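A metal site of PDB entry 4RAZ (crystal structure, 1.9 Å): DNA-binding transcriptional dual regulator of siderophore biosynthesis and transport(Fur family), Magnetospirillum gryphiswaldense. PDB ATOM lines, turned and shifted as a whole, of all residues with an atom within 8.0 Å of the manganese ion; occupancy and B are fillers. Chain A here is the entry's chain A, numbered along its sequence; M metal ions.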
ATOM      1  N   ALA A  33     -10.542  11.586   6.603  1.00  0.00           N
ATOM      2  CA  ALA A  33     -10.629  10.491   7.559  1.00  0.00           C
ATOM      3  C   ALA A  33      -9.752  10.751   8.805  1.00  0.00           C
ATOM      4  O   ALA A  33      -9.624   9.901   9.666  1.00  0.00           O
ATOM      5  CB  ALA A  33     -10.255   9.169   6.894  1.00  0.00           C
ATOM      6  N   ASP A  34      -9.204  11.953   8.902  1.00  0.00           N
ATOM      7  CA  ASP A  34      -8.245  12.286   9.959  1.00  0.00           C
ATOM      8  C   ASP A  34      -8.776  13.244  11.030  1.00  0.00           C
ATOM      9  O   ASP A  34      -7.998  13.942  11.697  1.00  0.00           O
ATOM     10  CB  ASP A  34      -6.980  12.869   9.333  1.00  0.00           C
ATOM     11  CG  ASP A  34      -7.272  14.013   8.350  1.00  0.00           C
ATOM     12  OD1 ASP A  34      -6.276  14.559   7.829  1.00  0.00           O
ATOM     13  OD2 ASP A  34      -8.462  14.353   8.088  1.00  0.00           O
ATOM     14  N   HIS A  35     -10.104  13.286  11.183  1.00  0.00           N
ATOM     15  CA  HIS A  35     -10.776  14.116  12.200  1.00  0.00           C
ATOM     16  C   HIS A  35     -10.230  15.515  12.183  1.00  0.00           C
ATOM     17  O   HIS A  35      -9.661  15.983  13.176  1.00  0.00           O
ATOM     18  CB  HIS A  35     -10.654  13.489  13.594  1.00  0.00           C
ATOM     19  CG  HIS A  35     -11.253  12.082  13.686  1.00  0.00           C
ATOM     20  ND1 HIS A  35     -10.646  10.996  13.150  1.00  0.00           N
ATOM     21  CD2 HIS A  35     -12.412  11.626  14.313  1.00  0.00           C
ATOM     22  CE1 HIS A  35     -11.404   9.887  13.391  1.00  0.00           C
ATOM     23  NE2 HIS A  35     -12.485  10.271  14.122  1.00  0.00           N
ATOM     24  N   GLU A  71     -20.217  14.974  13.741  1.00  0.00           N
ATOM     25  CA  GLU A  71     -19.983  14.916  15.162  1.00  0.00           C
ATOM     26  C   GLU A  71     -18.753  15.756  15.499  1.00  0.00           C
ATOM     27  O   GLU A  71     -17.755  15.721  14.780  1.00  0.00           O
ATOM     28  CB  GLU A  71     -19.780  13.467  15.592  1.00  0.00           C
ATOM     29  CG  GLU A  71     -19.844  13.289  17.098  1.00  0.00           C
ATOM     30  CD  GLU A  71     -19.623  11.859  17.519  1.00  0.00           C
ATOM     31  OE1 GLU A  71     -19.420  11.628  18.736  1.00  0.00           O
ATOM     32  OE2 GLU A  71     -19.640  10.983  16.637  1.00  0.00           O
ATOM     33  N   HIS A  73     -15.664  16.516  18.255  1.00  0.00           N
ATOM     34  CA  HIS A  73     -14.869  15.993  19.381  1.00  0.00           C
ATOM     35  C   HIS A  73     -13.944  17.022  19.911  1.00  0.00           C
ATOM     36  O   HIS A  73     -13.383  17.829  19.149  1.00  0.00           O
ATOM     37  CB  HIS A  73     -14.038  14.774  18.951  1.00  0.00           C
ATOM     38  CG  HIS A  73     -14.860  13.620  18.500  1.00  0.00           C
ATOM     39  ND1 HIS A  73     -15.489  12.805  19.351  1.00  0.00           N
ATOM     40  CD2 HIS A  73     -15.174  13.178  17.209  1.00  0.00           C
ATOM     41  CE1 HIS A  73     -16.175  11.876  18.655  1.00  0.00           C
ATOM     42  NE2 HIS A  73     -15.967  12.103  17.339  1.00  0.00           N
ATOM     43  N   PHE A  75     -10.757  16.366  22.335  1.00  0.00           N
ATOM     44  CA  PHE A  75     -10.005  15.298  22.992  1.00  0.00           C
ATOM     45  C   PHE A  75      -9.221  15.780  24.220  1.00  0.00           C
ATOM     46  O   PHE A  75      -8.324  15.101  24.681  1.00  0.00           O
ATOM     47  CB  PHE A  75      -9.104  14.570  21.978  1.00  0.00           C
ATOM     48  CG  PHE A  75      -9.871  13.863  20.879  1.00  0.00           C
ATOM     49  CD1 PHE A  75     -10.865  12.948  21.195  1.00  0.00           C
ATOM     50  CD2 PHE A  75      -9.583  14.125  19.532  1.00  0.00           C
ATOM     51  CE1 PHE A  75     -11.588  12.283  20.189  1.00  0.00           C
ATOM     52  CE2 PHE A  75     -10.292  13.457  18.526  1.00  0.00           C
ATOM     53  CZ  PHE A  75     -11.294  12.542  18.849  1.00  0.00           C
ATOM     54  N   TYR A  82     -13.693  17.151  13.831  1.00  0.00           N
ATOM     55  CA  TYR A  82     -14.956  16.735  13.209  1.00  0.00           C
ATOM     56  C   TYR A  82     -14.868  15.517  12.310  1.00  0.00           C
ATOM     57  O   TYR A  82     -13.863  15.267  11.650  1.00  0.00           O
ATOM     58  CB  TYR A  82     -15.518  17.909  12.362  1.00  0.00           C
ATOM     59  CG  TYR A  82     -15.841  19.133  13.168  1.00  0.00           C
ATOM     60  CD1 TYR A  82     -17.118  19.316  13.722  1.00  0.00           C
ATOM     61  CD2 TYR A  82     -14.873  20.103  13.402  1.00  0.00           C
ATOM     62  CE1 TYR A  82     -17.405  20.429  14.488  1.00  0.00           C
ATOM     63  CE2 TYR A  82     -15.164  21.231  14.150  1.00  0.00           C
ATOM     64  CZ  TYR A  82     -16.423  21.392  14.693  1.00  0.00           C
ATOM     65  OH  TYR A  82     -16.689  22.505  15.439  1.00  0.00           O
ATOM     66  N   GLU A  83     -15.971  14.789  12.264  1.00  0.00           N
ATOM     67  CA  GLU A  83     -16.129  13.675  11.353  1.00  0.00           C
ATOM     68  C   GLU A  83     -17.603  13.529  11.030  1.00  0.00           C
ATOM     69  O   GLU A  83     -18.458  13.964  11.802  1.00  0.00           O
ATOM     70  CB  GLU A  83     -15.621  12.400  12.019  1.00  0.00           C
ATOM     71  CG  GLU A  83     -16.292  12.098  13.362  1.00  0.00           C
ATOM     72  CD  GLU A  83     -15.806  10.776  13.942  1.00  0.00           C
ATOM     73  OE1 GLU A  83     -15.653   9.822  13.154  1.00  0.00           O
ATOM     74  OE2 GLU A  83     -15.527  10.709  15.160  1.00  0.00           O
ATOM     75  N   GLU A  84     -17.914  12.896   9.912  1.00  0.00           N
ATOM     76  CA  GLU A  84     -19.306  12.582   9.611  1.00  0.00           C
ATOM     77  C   GLU A  84     -19.904  11.797  10.733  1.00  0.00           C
ATOM     78  O   GLU A  84     -19.234  10.933  11.311  1.00  0.00           O
ATOM     79  CB  GLU A  84     -19.369  11.672   8.398  1.00  0.00           C
ATOM     80  CG  GLU A  84     -18.894  12.300   7.122  1.00  0.00           C
ATOM     81  CD  GLU A  84     -18.790  11.254   6.025  1.00  0.00           C
ATOM     82  OE1 GLU A  84     -17.670  11.053   5.537  1.00  0.00           O
ATOM     83  OE2 GLU A  84     -19.815  10.610   5.712  1.00  0.00           O
ATOM     84  N   PRO A  86     -21.034   9.013  12.618  1.00  0.00           N
ATOM     85  CA  PRO A  86     -20.695   7.614  12.326  1.00  0.00           C
ATOM     86  C   PRO A  86     -21.945   6.762  12.262  1.00  0.00           C
ATOM     87  O   PRO A  86     -22.910   7.035  12.967  1.00  0.00           O
ATOM     88  CB  PRO A  86     -19.858   7.165  13.545  1.00  0.00           C
ATOM     89  CG  PRO A  86     -19.504   8.413  14.274  1.00  0.00           C
ATOM     90  CD  PRO A  86     -20.584   9.415  13.966  1.00  0.00           C
ATOM     91  N   GLU A  88     -21.634   3.436  12.810  1.00  0.00           N
ATOM     92  CA  GLU A  88     -21.359   2.430  13.839  1.00  0.00           C
ATOM     93  C   GLU A  88     -20.616   3.133  14.972  1.00  0.00           C
ATOM     94  O   GLU A  88     -19.748   3.961  14.721  1.00  0.00           O
ATOM     95  CB  GLU A  88     -20.498   1.279  13.282  1.00  0.00           C
ATOM     96  CG  GLU A  88     -20.950   0.688  11.939  1.00  0.00           C
ATOM     97  CD  GLU A  88     -22.016  -0.385  12.067  1.00  0.00           C
ATOM     98  OE2 GLU A  88     -23.084  -0.127  12.660  1.00  0.00           O
ATOM     99  N   HIS A  89     -20.959   2.804  16.212  1.00  0.00           N
ATOM    100  CA  HIS A  89     -20.225   3.348  17.357  1.00  0.00           C
ATOM    101  C   HIS A  89     -18.742   2.977  17.346  1.00  0.00           C
ATOM    102  O   HIS A  89     -18.393   1.842  17.000  1.00  0.00           O
ATOM    103  CB  HIS A  89     -20.883   2.927  18.664  1.00  0.00           C
ATOM    104  CG  HIS A  89     -20.081   3.315  19.878  1.00  0.00           C
ATOM    105  ND1 HIS A  89     -19.971   4.587  20.285  1.00  0.00           N
ATOM    106  CD2 HIS A  89     -19.272   2.554  20.730  1.00  0.00           C
ATOM    107  CE1 HIS A  89     -19.167   4.649  21.370  1.00  0.00           C
ATOM    108  NE2 HIS A  89     -18.742   3.398  21.635  1.00  0.00           N
ATOM    109  N   HIS A  90     -17.873   3.927  17.693  1.00  0.00           N
ATOM    110  CA  HIS A  90     -16.453   3.650  17.941  1.00  0.00           C
ATOM    111  C   HIS A  90     -15.899   4.627  18.967  1.00  0.00           C
ATOM    112  O   HIS A  90     -16.519   5.663  19.250  1.00  0.00           O
ATOM    113  CB  HIS A  90     -15.626   3.691  16.640  1.00  0.00           C
ATOM    114  CG  HIS A  90     -15.673   5.033  15.931  1.00  0.00           C
ATOM    115  ND1 HIS A  90     -16.599   5.313  14.994  1.00  0.00           N
ATOM    116  CD2 HIS A  90     -14.904   6.193  16.104  1.00  0.00           C
ATOM    117  CE1 HIS A  90     -16.447   6.586  14.573  1.00  0.00           C
ATOM    118  NE2 HIS A  90     -15.405   7.127  15.241  1.00  0.00           N
ATOM    119  N   ASP A  91     -14.750   4.283  19.524  1.00  0.00           N
ATOM    120  CA  ASP A  91     -14.055   5.160  20.463  1.00  0.00           C
ATOM    121  C   ASP A  91     -12.766   5.576  19.812  1.00  0.00           C
ATOM    122  O   ASP A  91     -12.507   5.197  18.659  1.00  0.00           O
ATOM    123  CB  ASP A  91     -13.846   4.425  21.800  1.00  0.00           C
ATOM    124  CG  ASP A  91     -15.138   3.874  22.323  1.00  0.00           C
ATOM    125  OD1 ASP A  91     -15.981   4.675  22.798  1.00  0.00           O
ATOM    126  OD2 ASP A  91     -15.360   2.644  22.255  1.00  0.00           O
ATOM    127  N   HIS A  92     -11.972   6.391  20.501  1.00  0.00           N
ATOM    128  CA  HIS A  92     -10.756   6.953  19.910  1.00  0.00           C
ATOM    129  C   HIS A  92      -9.535   6.812  20.776  1.00  0.00           C
ATOM    130  O   HIS A  92      -9.578   7.007  21.993  1.00  0.00           O
ATOM    131  CB  HIS A  92     -10.969   8.430  19.588  1.00  0.00           C
ATOM    132  CG  HIS A  92     -12.113   8.663  18.633  1.00  0.00           C
ATOM    133  ND1 HIS A  92     -13.393   8.746  19.047  1.00  0.00           N
ATOM    134  CD2 HIS A  92     -12.140   8.749  17.232  1.00  0.00           C
ATOM    135  CE1 HIS A  92     -14.209   8.914  17.973  1.00  0.00           C
ATOM    136  NE2 HIS A  92     -13.445   8.906  16.868  1.00  0.00           N
ATOM    137  N   VAL A 101      -5.350  10.551  15.231  1.00  0.00           N
ATOM    138  CA  VAL A 101      -6.500   9.854  15.844  1.00  0.00           C
ATOM    139  C   VAL A 101      -6.736   8.479  15.238  1.00  0.00           C
ATOM    140  O   VAL A 101      -6.798   8.328  14.010  1.00  0.00           O
ATOM    141  CB  VAL A 101      -7.803  10.731  15.791  1.00  0.00           C
ATOM    142  CG1 VAL A 101      -9.010   9.952  16.280  1.00  0.00           C
ATOM    143  CG2 VAL A 101      -7.630  11.986  16.635  1.00  0.00           C
ATOM    144  N   ILE A 102      -6.848   7.470  16.081  1.00  0.00           N
ATOM    145  CA  ILE A 102      -7.138   6.126  15.639  1.00  0.00           C
ATOM    146  C   ILE A 102      -8.481   5.687  16.215  1.00  0.00           C
ATOM    147  O   ILE A 102      -8.741   5.844  17.417  1.00  0.00           O
ATOM    148  CB  ILE A 102      -6.045   5.126  16.094  1.00  0.00           C
ATOM    149  CG1 ILE A 102      -4.723   5.490  15.419  1.00  0.00           C
ATOM    150  CG2 ILE A 102      -6.463   3.693  15.819  1.00  0.00           C
ATOM    151  CD1 ILE A 102      -3.504   4.809  16.009  1.00  0.00           C
ATOM    152  N   GLU A 103      -9.346   5.155  15.371  1.00  0.00           N
ATOM    153  CA  GLU A 103     -10.639   4.671  15.838  1.00  0.00           C
ATOM    154  C   GLU A 103     -10.569   3.202  16.240  1.00  0.00           C
ATOM    155  O   GLU A 103      -9.887   2.414  15.591  1.00  0.00           O
ATOM    156  CB  GLU A 103     -11.698   4.848  14.750  1.00  0.00           C
ATOM    157  CG  GLU A 103     -11.825   6.315  14.315  1.00  0.00           C
ATOM    158  CD  GLU A 103     -12.862   6.530  13.224  1.00  0.00           C
ATOM    159  OE1 GLU A 103     -13.141   5.585  12.484  1.00  0.00           O
ATOM    160  OE2 GLU A 103     -13.409   7.651  13.116  1.00  0.00           O
ATOM    161  N   PHE A 104     -11.316   2.819  17.260  1.00  0.00           N
ATOM    162  CA  PHE A 104     -11.408   1.408  17.637  1.00  0.00           C
ATOM    163  C   PHE A 104     -12.771   1.048  18.209  1.00  0.00           C
ATOM    164  O   PHE A 104     -13.533   1.927  18.642  1.00  0.00           O
ATOM    165  CB  PHE A 104     -10.280   1.026  18.657  1.00  0.00           C
ATOM    166  CG  PHE A 104     -10.488   1.601  20.035  1.00  0.00           C
ATOM    167  CD1 PHE A 104     -11.256   0.932  20.993  1.00  0.00           C
ATOM    168  CD2 PHE A 104      -9.890   2.821  20.394  1.00  0.00           C
ATOM    169  CE1 PHE A 104     -11.434   1.468  22.254  1.00  0.00           C
ATOM    170  CE2 PHE A 104     -10.056   3.351  21.669  1.00  0.00           C
ATOM    171  CZ  PHE A 104     -10.825   2.670  22.594  1.00  0.00           C
HETATM  172 MN    MN M   1     -14.114   8.903  14.734  1.00  0.00          MN
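The side-chain carboxylate (OE2) of Glu 83 sits close to a ring nitrogen (NE2) of His 73, 2.6 Å away.
O of Glu 88 lies within hydrogen-bond range of ND1 of His 90, 3.4 Å away.
N of Glu 71 is in hydrogen-bond range of O of Glu 83, at 2.8 Å.
Within 4 Å of the manganese ion: His 35, Glu 83, His 90, His 92 and Glu 103.
The nearest printed residue that does not touch the manganese ion is His 73 (4.5 Å).
The manganese ion is bound by the side-chain carboxylate (OE2) of Glu 103 (2.2 Å), a ring nitrogen (NE2) of His 35 (2.2 Å), a ring nitrogen (NE2) of His 92 (2.2 Å), a ring nitrogen (NE2) of His 90 (2.3 Å), the side-chain carboxylate (OE2) of Glu 83 (2.3 Å) and the side-chain carboxylate (OE1) of Glu 83 (2.4 Å).
The manganese ion has six donor atoms within binding distance.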
